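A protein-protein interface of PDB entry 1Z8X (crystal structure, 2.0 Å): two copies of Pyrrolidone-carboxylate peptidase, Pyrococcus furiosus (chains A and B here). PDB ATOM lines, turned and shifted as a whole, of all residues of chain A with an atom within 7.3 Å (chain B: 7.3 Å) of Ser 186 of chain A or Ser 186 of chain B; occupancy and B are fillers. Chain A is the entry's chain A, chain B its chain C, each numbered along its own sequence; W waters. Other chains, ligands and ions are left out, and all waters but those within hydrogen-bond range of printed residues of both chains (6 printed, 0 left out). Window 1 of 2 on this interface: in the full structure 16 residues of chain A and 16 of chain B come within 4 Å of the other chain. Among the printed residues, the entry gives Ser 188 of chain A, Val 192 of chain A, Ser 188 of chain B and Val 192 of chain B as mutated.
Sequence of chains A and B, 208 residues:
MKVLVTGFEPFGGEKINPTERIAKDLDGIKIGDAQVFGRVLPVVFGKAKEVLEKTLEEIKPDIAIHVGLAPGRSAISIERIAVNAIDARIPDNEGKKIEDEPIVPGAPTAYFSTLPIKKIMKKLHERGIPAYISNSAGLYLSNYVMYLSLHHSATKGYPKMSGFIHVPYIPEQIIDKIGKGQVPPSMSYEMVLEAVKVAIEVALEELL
Water W1 lies within hydrogen-bond range of O of Ser 186 of chain A, O of Ser 74 of chain A and N of Ser 186 of chain B.
Of chain B, only Ser 186 (3.2 Å) comes within 4 Å of Ser 186 of chain A.
Ser 186 of chain B touches one residue of chain A.
Printed residues of chain A within 4 Å of Ile 174 of chain B: Pro 130 (3.8 Å).
Of the printed residues of chain A, Met 191 of chain B touches Pro 171.
Tyr 169 of chain A touches none of the printed residues of chain B.
Pro 168 of chain A touches none of the printed residues of chain B.
The nearest residue of chain B that does not touch Ser 186 of chain A is Pro 130 of chain B (4.1 Å).
The nearest residue of chain A that does not touch Ser 186 of chain B is Pro 130 of chain A (4.1 Å).
The nearest printed residue of chain B that does not touch Met 191 of chain A is Ser 186 of chain B (6.1 Å).
Among the printed residues, pairs that only touch across the chains: Ser 74 of chain A with Pro 184 of chain B (3.9 Å), Ala 75 of chain A with Val 183 of chain B (3.7 Å), Pro 130 of chain A with Pro 171 of chain B (3.6 Å), Pro 130 of chain A with Ile 174 of chain B (3.8 Å), Pro 171 of chain A with Pro 130 of chain B (3.6 Å), Pro 171 of chain A with Met 191 of chain B (3.7 Å), Ile 174 of chain A with Pro 130 of chain B (3.8 Å), Val 183 of chain A with Ala 75 of chain B (3.7 Å), Pro 184 of chain A with Ser 74 of chain B (3.97 Å), Pro 185 of chain A with Pro 185 of chain B (3.9 Å) and Met 191 of chain A with Pro 171 of chain B (3.7 Å).
Hydrophobic or aromatic side chains of chain A within 4 Å of the printed part of chain B: Ala 75, Pro 130, Pro 171, Ile 174, Val 183, Pro 185 and Met 191.
Hydrophobic or aromatic side chains of chain B within 4 Å of the printed part of chain A: Ala 75, Pro 130, Pro 171, Ile 174, Val 183, Pro 185 and Met 191.
The side-chain hydroxyl (OG) of Ser 188 of chain A sits at hydrogen-bond distance from the backbone NH (N) of Met 191 of chain A (3.0 Å).
The backbone NH (N) of Met 191 of chain B is in hydrogen-bond range of the side-chain hydroxyl (OG) of Ser 188 of chain B (3.0 Å).
The side-chain hydroxyl (OG) of Ser 74 of chain A is in hydrogen-bond range of the backbone carbonyl oxygen (O) of Val 183 of chain B (2.7 Å).
The side-chain hydroxyl (OG) of Ser 74 of chain B sits at hydrogen-bond distance from the backbone carbonyl oxygen (O) of Val 183 of chain A.
The backbone carbonyl oxygen (O) of Ser 186 of chain A lies close to the backbone carbonyl oxygen (O) of Ser 186 of chain B (3.2 Å).
Pro 130 of chain A touches Ile 174 of chain B, and with the chains exchanged Ile 174 of chain A touches Pro 130 of chain B.
Pro 185 of chain A touches its own counterpart, Pro 185 of chain B.
Positions printed for both chains: 72, 73, 74, 75, 130, 168, 169, 170, 171, 172, 173, 174, 183, 184, 185, 186, 187, 188, 191 and 192.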
ATOM      1  N   GLY A  72     -24.061 -14.915  12.731  1.00  0.00           N
ATOM      2  CA  GLY A  72     -22.864 -14.528  13.452  1.00  0.00           C
ATOM      3  C   GLY A  72     -22.208 -13.248  12.988  1.00  0.00           C
ATOM      4  O   GLY A  72     -21.478 -12.618  13.754  1.00  0.00           O
ATOM      5  N   ARG A  73     -22.433 -12.855  11.737  1.00  0.00           N
ATOM      6  CA  ARG A  73     -21.827 -11.619  11.261  1.00  0.00           C
ATOM      7  C   ARG A  73     -22.532 -10.419  11.893  1.00  0.00           C
ATOM      8  O   ARG A  73     -23.749 -10.422  12.080  1.00  0.00           O
ATOM      9  CB  ARG A  73     -21.820 -11.594   9.729  1.00  0.00           C
ATOM     10  CG  ARG A  73     -20.494 -12.173   9.219  1.00  0.00           C
ATOM     11  CD  ARG A  73     -20.595 -13.132   8.060  1.00  0.00           C
ATOM     12  NE  ARG A  73     -20.506 -12.458   6.777  1.00  0.00           N
ATOM     13  CZ  ARG A  73     -19.861 -12.938   5.715  1.00  0.00           C
ATOM     14  NH1 ARG A  73     -19.230 -14.104   5.774  1.00  0.00           N
ATOM     15  NH2 ARG A  73     -19.865 -12.255   4.581  1.00  0.00           N
ATOM     16  N   SER A  74     -21.746  -9.405  12.240  1.00  0.00           N
ATOM     17  CA  SER A  74     -22.249  -8.224  12.942  1.00  0.00           C
ATOM     18  C   SER A  74     -22.681  -7.035  12.104  1.00  0.00           C
ATOM     19  O   SER A  74     -23.259  -6.085  12.631  1.00  0.00           O
ATOM     20  CB  SER A  74     -21.184  -7.750  13.927  1.00  0.00           C
ATOM     21  OG  SER A  74     -20.020  -7.362  13.216  1.00  0.00           O
ATOM     22  N   ALA A  75     -22.394  -7.066  10.814  1.00  0.00           N
ATOM     23  CA  ALA A  75     -22.761  -5.947   9.960  1.00  0.00           C
ATOM     24  C   ALA A  75     -23.018  -6.442   8.551  1.00  0.00           C
ATOM     25  O   ALA A  75     -22.797  -7.610   8.246  1.00  0.00           O
ATOM     26  CB  ALA A  75     -21.634  -4.918   9.941  1.00  0.00           C
ATOM     27  N   PRO A 130     -23.573   0.017   9.360  1.00  0.00           N
ATOM     28  CA  PRO A 130     -22.286  -0.684   9.394  1.00  0.00           C
ATOM     29  C   PRO A 130     -22.192  -1.712   8.268  1.00  0.00           C
ATOM     30  O   PRO A 130     -23.123  -2.484   8.030  1.00  0.00           O
ATOM     31  CB  PRO A 130     -22.242  -1.312  10.799  1.00  0.00           C
ATOM     32  CG  PRO A 130     -23.637  -1.149  11.356  1.00  0.00           C
ATOM     33  CD  PRO A 130     -24.187   0.080  10.698  1.00  0.00           C
ATOM     34  N   PRO A 168     -26.814  -9.870   8.701  1.00  0.00           N
ATOM     35  CA  PRO A 168     -26.772 -10.510  10.016  1.00  0.00           C
ATOM     36  C   PRO A 168     -28.152 -11.053  10.365  1.00  0.00           C
ATOM     37  O   PRO A 168     -29.116 -10.856   9.616  1.00  0.00           O
ATOM     38  CB  PRO A 168     -26.399  -9.358  10.954  1.00  0.00           C
ATOM     39  CG  PRO A 168     -25.704  -8.373  10.066  1.00  0.00           C
ATOM     40  CD  PRO A 168     -26.529  -8.430   8.807  1.00  0.00           C
ATOM     41  N   TYR A 169     -28.241 -11.740  11.498  1.00  0.00           N
ATOM     42  CA  TYR A 169     -29.521 -12.231  11.997  1.00  0.00           C
ATOM     43  C   TYR A 169     -30.294 -10.962  12.341  1.00  0.00           C
ATOM     44  O   TYR A 169     -29.680  -9.934  12.637  1.00  0.00           O
ATOM     45  CB  TYR A 169     -29.351 -12.958  13.333  1.00  0.00           C
ATOM     46  CG  TYR A 169     -28.892 -14.394  13.320  1.00  0.00           C
ATOM     47  CD1 TYR A 169     -29.635 -15.382  12.681  1.00  0.00           C
ATOM     48  CD2 TYR A 169     -27.772 -14.783  14.063  1.00  0.00           C
ATOM     49  CE1 TYR A 169     -29.282 -16.738  12.792  1.00  0.00           C
ATOM     50  CE2 TYR A 169     -27.414 -16.124  14.181  1.00  0.00           C
ATOM     51  CZ  TYR A 169     -28.178 -17.095  13.544  1.00  0.00           C
ATOM     52  OH  TYR A 169     -27.845 -18.424  13.682  1.00  0.00           O
ATOM     53  N   ILE A 170     -31.625 -11.012  12.306  1.00  0.00           N
ATOM     54  CA  ILE A 170     -32.391  -9.852  12.756  1.00  0.00           C
ATOM     55  C   ILE A 170     -32.700 -10.223  14.219  1.00  0.00           C
ATOM     56  O   ILE A 170     -32.690 -11.401  14.573  1.00  0.00           O
ATOM     57  CB  ILE A 170     -33.683  -9.610  11.927  1.00  0.00           C
ATOM     58  CG1 ILE A 170     -34.542 -10.867  11.870  1.00  0.00           C
ATOM     59  CG2 ILE A 170     -33.302  -9.148  10.517  1.00  0.00           C
ATOM     60  CD1 ILE A 170     -35.851 -10.651  11.132  1.00  0.00           C
ATOM     61  N   PRO A 171     -32.948  -9.227  15.088  1.00  0.00           N
ATOM     62  CA  PRO A 171     -33.233  -9.446  16.515  1.00  0.00           C
ATOM     63  C   PRO A 171     -34.148 -10.602  16.934  1.00  0.00           C
ATOM     64  O   PRO A 171     -33.797 -11.370  17.828  1.00  0.00           O
ATOM     65  CB  PRO A 171     -33.768  -8.090  16.974  1.00  0.00           C
ATOM     66  CG  PRO A 171     -33.007  -7.128  16.100  1.00  0.00           C
ATOM     67  CD  PRO A 171     -33.095  -7.802  14.744  1.00  0.00           C
ATOM     68  N   GLU A 172     -35.313 -10.729  16.308  1.00  0.00           N
ATOM     69  CA  GLU A 172     -36.239 -11.797  16.676  1.00  0.00           C
ATOM     70  C   GLU A 172     -35.651 -13.199  16.529  1.00  0.00           C
ATOM     71  O   GLU A 172     -36.114 -14.140  17.175  1.00  0.00           O
ATOM     72  CB  GLU A 172     -37.526 -11.695  15.858  1.00  0.00           C
ATOM     73  CG  GLU A 172     -37.311 -11.617  14.360  1.00  0.00           C
ATOM     74  CD  GLU A 172     -38.574 -11.246  13.613  1.00  0.00           C
ATOM     75  OE1 GLU A 172     -39.389 -12.151  13.327  1.00  0.00           O
ATOM     76  OE2 GLU A 172     -38.758 -10.041  13.324  1.00  0.00           O
ATOM     77  N   GLN A 173     -34.633 -13.338  15.683  1.00  0.00           N
ATOM     78  CA  GLN A 173     -34.000 -14.636  15.478  1.00  0.00           C
ATOM     79  C   GLN A 173     -33.068 -15.011  16.631  1.00  0.00           C
ATOM     80  O   GLN A 173     -32.711 -16.175  16.790  1.00  0.00           O
ATOM     81  CB  GLN A 173     -33.198 -14.637  14.172  1.00  0.00           C
ATOM     82  CG  GLN A 173     -34.038 -14.570  12.907  1.00  0.00           C
ATOM     83  CD  GLN A 173     -33.191 -14.687  11.648  1.00  0.00           C
ATOM     84  OE1 GLN A 173     -32.512 -13.739  11.244  1.00  0.00           O
ATOM     85  NE2 GLN A 173     -33.212 -15.866  11.034  1.00  0.00           N
ATOM     86  N   ILE A 174     -32.681 -14.021  17.432  1.00  0.00           N
ATOM     87  CA  ILE A 174     -31.772 -14.244  18.551  1.00  0.00           C
ATOM     88  C   ILE A 174     -32.456 -14.777  19.814  1.00  0.00           C
ATOM     89  O   ILE A 174     -31.844 -15.501  20.601  1.00  0.00           O
ATOM     90  CB  ILE A 174     -31.038 -12.936  18.930  1.00  0.00           C
ATOM     91  CG1 ILE A 174     -30.365 -12.328  17.692  1.00  0.00           C
ATOM     92  CG2 ILE A 174     -30.012 -13.214  20.022  1.00  0.00           C
ATOM     93  CD1 ILE A 174     -29.337 -13.233  17.035  1.00  0.00           C
ATOM     94  N   VAL A 183     -25.161 -15.515  22.557  1.00  0.00           N
ATOM     95  CA  VAL A 183     -25.871 -14.400  21.949  1.00  0.00           C
ATOM     96  C   VAL A 183     -25.166 -13.795  20.734  1.00  0.00           C
ATOM     97  O   VAL A 183     -24.326 -12.901  20.860  1.00  0.00           O
ATOM     98  CB  VAL A 183     -26.123 -13.282  22.975  1.00  0.00           C
ATOM     99  CG1 VAL A 183     -27.113 -12.285  22.410  1.00  0.00           C
ATOM    100  CG2 VAL A 183     -26.644 -13.874  24.279  1.00  0.00           C
ATOM    101  N   PRO A 184     -25.506 -14.277  19.533  1.00  0.00           N
ATOM    102  CA  PRO A 184     -24.867 -13.730  18.337  1.00  0.00           C
ATOM    103  C   PRO A 184     -25.352 -12.312  18.025  1.00  0.00           C
ATOM    104  O   PRO A 184     -26.385 -11.870  18.526  1.00  0.00           O
ATOM    105  CB  PRO A 184     -25.245 -14.739  17.247  1.00  0.00           C
ATOM    106  CG  PRO A 184     -26.547 -15.282  17.709  1.00  0.00           C
ATOM    107  CD  PRO A 184     -26.345 -15.445  19.202  1.00  0.00           C
ATOM    108  N   PRO A 185     -24.589 -11.573  17.206  1.00  0.00           N
ATOM    109  CA  PRO A 185     -24.921 -10.198  16.809  1.00  0.00           C
ATOM    110  C   PRO A 185     -26.180 -10.181  15.946  1.00  0.00           C
ATOM    111  O   PRO A 185     -26.530 -11.194  15.344  1.00  0.00           O
ATOM    112  CB  PRO A 185     -23.699  -9.763  15.997  1.00  0.00           C
ATOM    113  CG  PRO A 185     -22.595 -10.632  16.522  1.00  0.00           C
ATOM    114  CD  PRO A 185     -23.262 -11.961  16.702  1.00  0.00           C
ATOM    115  N   SER A 186     -26.850  -9.037  15.888  1.00  0.00           N
ATOM    116  CA  SER A 186     -28.046  -8.893  15.070  1.00  0.00           C
ATOM    117  C   SER A 186     -28.146  -7.466  14.531  1.00  0.00           C
ATOM    118  O   SER A 186     -27.422  -6.569  14.972  1.00  0.00           O
ATOM    119  CB  SER A 186     -29.304  -9.251  15.878  1.00  0.00           C
ATOM    120  OG  SER A 186     -29.433  -8.449  17.038  1.00  0.00           O
ATOM    121  N   MET A 187     -29.028  -7.277  13.554  1.00  0.00           N
ATOM    122  CA  MET A 187     -29.259  -5.977  12.935  1.00  0.00           C
ATOM    123  C   MET A 187     -30.747  -5.894  12.599  1.00  0.00           C
ATOM    124  O   MET A 187     -31.331  -6.879  12.139  1.00  0.00           O
ATOM    125  CB  MET A 187     -28.415  -5.840  11.665  1.00  0.00           C
ATOM    126  CG  MET A 187     -28.544  -4.486  10.972  1.00  0.00           C
ATOM    127  SD  MET A 187     -27.355  -4.286   9.610  1.00  0.00           S
ATOM    128  CE  MET A 187     -25.879  -3.833  10.514  1.00  0.00           C
ATOM    129  N   SER A 188     -31.362  -4.734  12.818  1.00  0.00           N
ATOM    130  CA  SER A 188     -32.799  -4.590  12.560  1.00  0.00           C
ATOM    131  C   SER A 188     -33.184  -4.941  11.133  1.00  0.00           C
ATOM    132  O   SER A 188     -32.412  -4.717  10.201  1.00  0.00           O
ATOM    133  CB  SER A 188     -33.272  -3.167  12.865  1.00  0.00           C
ATOM    134  OG  SER A 188     -32.895  -2.269  11.835  1.00  0.00           O
ATOM    135  N   MET A 191     -33.052  -1.958   8.826  1.00  0.00           N
ATOM    136  CA  MET A 191     -31.728  -1.569   8.358  1.00  0.00           C
ATOM    137  C   MET A 191     -31.221  -2.512   7.265  1.00  0.00           C
ATOM    138  O   MET A 191     -30.626  -2.070   6.283  1.00  0.00           O
ATOM    139  CB  MET A 191     -30.733  -1.535   9.519  1.00  0.00           C
ATOM    140  CG  MET A 191     -29.323  -1.163   9.078  1.00  0.00           C
ATOM    141  SD  MET A 191     -28.194  -0.776  10.413  1.00  0.00           S
ATOM    142  CE  MET A 191     -28.770   0.882  10.869  1.00  0.00           C
ATOM    143  N   VAL A 192     -31.449  -3.810   7.442  1.00  0.00           N
ATOM    144  CA  VAL A 192     -31.018  -4.790   6.454  1.00  0.00           C
ATOM    145  C   VAL A 192     -31.739  -4.556   5.124  1.00  0.00           C
ATOM    146  O   VAL A 192     -31.140  -4.658   4.055  1.00  0.00           O
ATOM    147  CB  VAL A 192     -31.291  -6.230   6.957  1.00  0.00           C
ATOM    148  CG1 VAL A 192     -31.149  -7.208   5.829  1.00  0.00           C
ATOM    149  CG2 VAL A 192     -30.311  -6.574   8.076  1.00  0.00           C
ATOM    150  N   GLY B  72     -19.008  -3.823  22.549  1.00  0.00           N
ATOM    151  CA  GLY B  72     -18.782  -5.221  22.238  1.00  0.00           C
ATOM    152  C   GLY B  72     -19.925  -6.160  22.570  1.00  0.00           C
ATOM    153  O   GLY B  72     -20.023  -7.246  21.994  1.00  0.00           O
ATOM    154  N   ARG B  73     -20.789  -5.774  23.503  1.00  0.00           N
ATOM    155  CA  ARG B  73     -21.901  -6.649  23.837  1.00  0.00           C
ATOM    156  C   ARG B  73     -22.935  -6.622  22.715  1.00  0.00           C
ATOM    157  O   ARG B  73     -23.198  -5.578  22.113  1.00  0.00           O
ATOM    158  CB  ARG B  73     -22.472  -6.281  25.213  1.00  0.00           C
ATOM    159  CG  ARG B  73     -21.772  -7.108  26.287  1.00  0.00           C
ATOM    160  CD  ARG B  73     -21.363  -6.374  27.541  1.00  0.00           C
ATOM    161  NE  ARG B  73     -22.406  -6.370  28.548  1.00  0.00           N
ATOM    162  CZ  ARG B  73     -22.190  -6.484  29.857  1.00  0.00           C
ATOM    163  NH1 ARG B  73     -20.960  -6.623  30.331  1.00  0.00           N
ATOM    164  NH2 ARG B  73     -23.211  -6.443  30.696  1.00  0.00           N
ATOM    165  N   SER B  74     -23.493  -7.792  22.422  1.00  0.00           N
ATOM    166  CA  SER B  74     -24.434  -7.959  21.312  1.00  0.00           C
ATOM    167  C   SER B  74     -25.918  -7.793  21.604  1.00  0.00           C
ATOM    168  O   SER B  74     -26.731  -7.764  20.679  1.00  0.00           O
ATOM    169  CB  SER B  74     -24.220  -9.338  20.697  1.00  0.00           C
ATOM    170  OG  SER B  74     -24.496 -10.336  21.666  1.00  0.00           O
ATOM    171  N   ALA B  75     -26.281  -7.700  22.876  1.00  0.00           N
ATOM    172  CA  ALA B  75     -27.676  -7.561  23.225  1.00  0.00           C
ATOM    173  C   ALA B  75     -27.815  -6.785  24.517  1.00  0.00           C
ATOM    174  O   ALA B  75     -26.824  -6.459  25.169  1.00  0.00           O
ATOM    175  CB  ALA B  75     -28.306  -8.941  23.376  1.00  0.00           C
ATOM    176  N   PRO B 130     -33.438  -8.856  21.956  1.00  0.00           N
ATOM    177  CA  PRO B 130     -32.461  -9.762  22.567  1.00  0.00           C
ATOM    178  C   PRO B 130     -31.911  -9.176  23.867  1.00  0.00           C
ATOM    179  O   PRO B 130     -31.552  -7.995  23.934  1.00  0.00           O
ATOM    180  CB  PRO B 130     -31.398  -9.939  21.475  1.00  0.00           C
ATOM    181  CG  PRO B 130     -31.709  -8.896  20.433  1.00  0.00           C
ATOM    182  CD  PRO B 130     -33.179  -8.677  20.518  1.00  0.00           C
ATOM    183  N   PRO B 168     -25.700  -2.166  23.881  1.00  0.00           N
ATOM    184  CA  PRO B 168     -24.634  -2.312  22.884  1.00  0.00           C
ATOM    185  C   PRO B 168     -24.397  -0.971  22.201  1.00  0.00           C
ATOM    186  O   PRO B 168     -25.112  -0.009  22.453  1.00  0.00           O
ATOM    187  CB  PRO B 168     -25.223  -3.315  21.883  1.00  0.00           C
ATOM    188  CG  PRO B 168     -26.255  -4.068  22.688  1.00  0.00           C
ATOM    189  CD  PRO B 168     -26.875  -2.973  23.516  1.00  0.00           C
ATOM    190  N   TYR B 169     -23.393  -0.923  21.335  1.00  0.00           N
ATOM    191  CA  TYR B 169     -23.114   0.270  20.545  1.00  0.00           C
ATOM    192  C   TYR B 169     -24.326   0.396  19.629  1.00  0.00           C
ATOM    193  O   TYR B 169     -24.977  -0.617  19.325  1.00  0.00           O
ATOM    194  CB  TYR B 169     -21.934   0.037  19.597  1.00  0.00           C
ATOM    195  CG  TYR B 169     -20.535   0.150  20.145  1.00  0.00           C
ATOM    196  CD1 TYR B 169     -20.074   1.346  20.696  1.00  0.00           C
ATOM    197  CD2 TYR B 169     -19.625  -0.897  19.983  1.00  0.00           C
ATOM    198  CE1 TYR B 169     -18.734   1.502  21.058  1.00  0.00           C
ATOM    199  CE2 TYR B 169     -18.288  -0.753  20.341  1.00  0.00           C
ATOM    200  CZ  TYR B 169     -17.849   0.454  20.875  1.00  0.00           C
ATOM    201  OH  TYR B 169     -16.521   0.614  21.195  1.00  0.00           O
ATOM    202  N   ILE B 170     -24.639   1.608  19.182  1.00  0.00           N
ATOM    203  CA  ILE B 170     -25.716   1.752  18.210  1.00  0.00           C
ATOM    204  C   ILE B 170     -24.942   1.795  16.878  1.00  0.00           C
ATOM    205  O   ILE B 170     -23.761   2.148  16.862  1.00  0.00           O
ATOM    206  CB  ILE B 170     -26.571   3.032  18.423  1.00  0.00           C
ATOM    207  CG1 ILE B 170     -25.688   4.281  18.483  1.00  0.00           C
ATOM    208  CG2 ILE B 170     -27.390   2.891  19.705  1.00  0.00           C
ATOM    209  CD1 ILE B 170     -26.497   5.556  18.607  1.00  0.00           C
ATOM    210  N   PRO B 171     -25.585   1.419  15.761  1.00  0.00           N
ATOM    211  CA  PRO B 171     -24.958   1.392  14.430  1.00  0.00           C
ATOM    212  C   PRO B 171     -24.015   2.518  14.017  1.00  0.00           C
ATOM    213  O   PRO B 171     -22.919   2.254  13.531  1.00  0.00           O
ATOM    214  CB  PRO B 171     -26.152   1.265  13.487  1.00  0.00           C
ATOM    215  CG  PRO B 171     -27.121   0.448  14.305  1.00  0.00           C
ATOM    216  CD  PRO B 171     -27.024   1.111  15.664  1.00  0.00           C
ATOM    217  N   GLU B 172     -24.427   3.769  14.197  1.00  0.00           N
ATOM    218  CA  GLU B 172     -23.580   4.895  13.796  1.00  0.00           C
ATOM    219  C   GLU B 172     -22.226   4.923  14.497  1.00  0.00           C
ATOM    220  O   GLU B 172     -21.277   5.525  13.999  1.00  0.00           O
ATOM    221  CB  GLU B 172     -24.310   6.219  14.031  1.00  0.00           C
ATOM    222  CG  GLU B 172     -24.868   6.384  15.432  1.00  0.00           C
ATOM    223  CD  GLU B 172     -25.800   7.577  15.549  1.00  0.00           C
ATOM    224  OE1 GLU B 172     -25.304   8.713  15.705  1.00  0.00           O
ATOM    225  OE2 GLU B 172     -27.035   7.379  15.467  1.00  0.00           O
ATOM    226  N   GLN B 173     -22.133   4.276  15.653  1.00  0.00           N
ATOM    227  CA  GLN B 173     -20.878   4.249  16.401  1.00  0.00           C
ATOM    228  C   GLN B 173     -19.880   3.255  15.804  1.00  0.00           C
ATOM    229  O   GLN B 173     -18.685   3.312  16.093  1.00  0.00           O
ATOM    230  CB  GLN B 173     -21.137   3.873  17.864  1.00  0.00           C
ATOM    231  CG  GLN B 173     -21.880   4.920  18.673  1.00  0.00           C
ATOM    232  CD  GLN B 173     -22.011   4.527  20.133  1.00  0.00           C
ATOM    233  OE1 GLN B 173     -22.834   3.677  20.491  1.00  0.00           O
ATOM    234  NE2 GLN B 173     -21.187   5.136  20.986  1.00  0.00           N
ATOM    235  N   ILE B 174     -20.378   2.338  14.981  1.00  0.00           N
ATOM    236  CA  ILE B 174     -19.535   1.318  14.363  1.00  0.00           C
ATOM    237  C   ILE B 174     -18.783   1.795  13.111  1.00  0.00           C
ATOM    238  O   ILE B 174     -17.699   1.298  12.798  1.00  0.00           O
ATOM    239  CB  ILE B 174     -20.376   0.083  13.958  1.00  0.00           C
ATOM    240  CG1 ILE B 174     -21.187  -0.424  15.158  1.00  0.00           C
ATOM    241  CG2 ILE B 174     -19.462  -1.015  13.421  1.00  0.00           C
ATOM    242  CD1 ILE B 174     -20.355  -0.860  16.340  1.00  0.00           C
ATOM    243  N   VAL B 183     -15.215  -5.145  13.491  1.00  0.00           N
ATOM    244  CA  VAL B 183     -16.621  -4.764  13.494  1.00  0.00           C
ATOM    245  C   VAL B 183     -17.411  -5.303  14.690  1.00  0.00           C
ATOM    246  O   VAL B 183     -17.918  -6.428  14.668  1.00  0.00           O
ATOM    247  CB  VAL B 183     -17.316  -5.222  12.198  1.00  0.00           C
ATOM    248  CG1 VAL B 183     -18.677  -4.566  12.088  1.00  0.00           C
ATOM    249  CG2 VAL B 183     -16.450  -4.873  10.991  1.00  0.00           C
ATOM    250  N   PRO B 184     -17.515  -4.504  15.757  1.00  0.00           N
ATOM    251  CA  PRO B 184     -18.264  -4.970  16.925  1.00  0.00           C
ATOM    252  C   PRO B 184     -19.771  -4.979  16.672  1.00  0.00           C
ATOM    253  O   PRO B 184     -20.262  -4.351  15.730  1.00  0.00           O
ATOM    254  CB  PRO B 184     -17.854  -3.982  18.020  1.00  0.00           C
ATOM    255  CG  PRO B 184     -17.542  -2.739  17.268  1.00  0.00           C
ATOM    256  CD  PRO B 184     -16.817  -3.238  16.042  1.00  0.00           C
ATOM    257  N   PRO B 185     -20.522  -5.714  17.504  1.00  0.00           N
ATOM    258  CA  PRO B 185     -21.983  -5.818  17.387  1.00  0.00           C
ATOM    259  C   PRO B 185     -22.647  -4.479  17.698  1.00  0.00           C
ATOM    260  O   PRO B 185     -22.064  -3.639  18.387  1.00  0.00           O
ATOM    261  CB  PRO B 185     -22.348  -6.864  18.445  1.00  0.00           C
ATOM    262  CG  PRO B 185     -21.094  -7.670  18.604  1.00  0.00           C
ATOM    263  CD  PRO B 185     -20.011  -6.621  18.543  1.00  0.00           C
ATOM    264  N   SER B 186     -23.863  -4.285  17.195  1.00  0.00           N
ATOM    265  CA  SER B 186     -24.607  -3.061  17.460  1.00  0.00           C
ATOM    266  C   SER B 186     -26.106  -3.362  17.542  1.00  0.00           C
ATOM    267  O   SER B 186     -26.557  -4.453  17.177  1.00  0.00           O
ATOM    268  CB  SER B 186     -24.335  -2.009  16.375  1.00  0.00           C
ATOM    269  OG  SER B 186     -24.654  -2.492  15.078  1.00  0.00           O
ATOM    270  N   MET B 187     -26.864  -2.392  18.046  1.00  0.00           N
ATOM    271  CA  MET B 187     -28.311  -2.510  18.188  1.00  0.00           C
ATOM    272  C   MET B 187     -28.889  -1.121  17.937  1.00  0.00           C
ATOM    273  O   MET B 187     -28.323  -0.127  18.391  1.00  0.00           O
ATOM    274  CB  MET B 187     -28.664  -2.993  19.602  1.00  0.00           C
ATOM    275  CG  MET B 187     -30.159  -3.211  19.829  1.00  0.00           C
ATOM    276  SD  MET B 187     -30.491  -3.962  21.416  1.00  0.00           S
ATOM    277  CE  MET B 187     -30.218  -5.707  21.049  1.00  0.00           C
ATOM    278  N   SER B 188     -30.010  -1.044  17.222  1.00  0.00           N
ATOM    279  CA  SER B 188     -30.607   0.250  16.896  1.00  0.00           C
ATOM    280  C   SER B 188     -30.921   1.082  18.127  1.00  0.00           C
ATOM    281  O   SER B 188     -31.254   0.545  19.183  1.00  0.00           O
ATOM    282  CB  SER B 188     -31.888   0.067  16.076  1.00  0.00           C
ATOM    283  OG  SER B 188     -32.977  -0.329  16.904  1.00  0.00           O
ATOM    284  N   MET B 191     -34.382   0.458  19.481  1.00  0.00           N
ATOM    285  CA  MET B 191     -34.540  -0.743  20.285  1.00  0.00           C
ATOM    286  C   MET B 191     -33.954  -0.563  21.690  1.00  0.00           C
ATOM    287  O   MET B 191     -34.545  -0.995  22.679  1.00  0.00           O
ATOM    288  CB  MET B 191     -33.888  -1.945  19.595  1.00  0.00           C
ATOM    289  CG  MET B 191     -34.021  -3.233  20.409  1.00  0.00           C
ATOM    290  SD  MET B 191     -33.558  -4.733  19.519  1.00  0.00           S
ATOM    291  CE  MET B 191     -35.039  -4.971  18.502  1.00  0.00           C
ATOM    292  N   VAL B 192     -32.793   0.078  21.776  1.00  0.00           N
ATOM    293  CA  VAL B 192     -32.162   0.307  23.066  1.00  0.00           C
ATOM    294  C   VAL B 192     -33.049   1.200  23.936  1.00  0.00           C
ATOM    295  O   VAL B 192     -33.213   0.956  25.135  1.00  0.00           O
ATOM    296  CB  VAL B 192     -30.768   0.949  22.887  1.00  0.00           C
ATOM    297  CG1 VAL B 192     -30.267   1.478  24.202  1.00  0.00           C
ATOM    298  CG2 VAL B 192     -29.788  -0.095  22.341  1.00  0.00           C
HETATM  299  O   HOH W   1     -24.645  -6.410  15.169  1.00  0.00           O
HETATM  300  O   HOH W   2     -22.509  -3.649  14.041  1.00  0.00           O
HETATM  301  O   HOH W   3     -26.036  -7.248  17.980  1.00  0.00           O
HETATM  302  O   HOH W   4     -28.321  -9.545  19.158  1.00  0.00           O
HETATM  303  O   HOH W   5     -29.288  -5.734  17.180  1.00  0.00           O
HETATM  304  O   HOH W   6     -27.064  -3.624  14.251  1.00  0.00           O
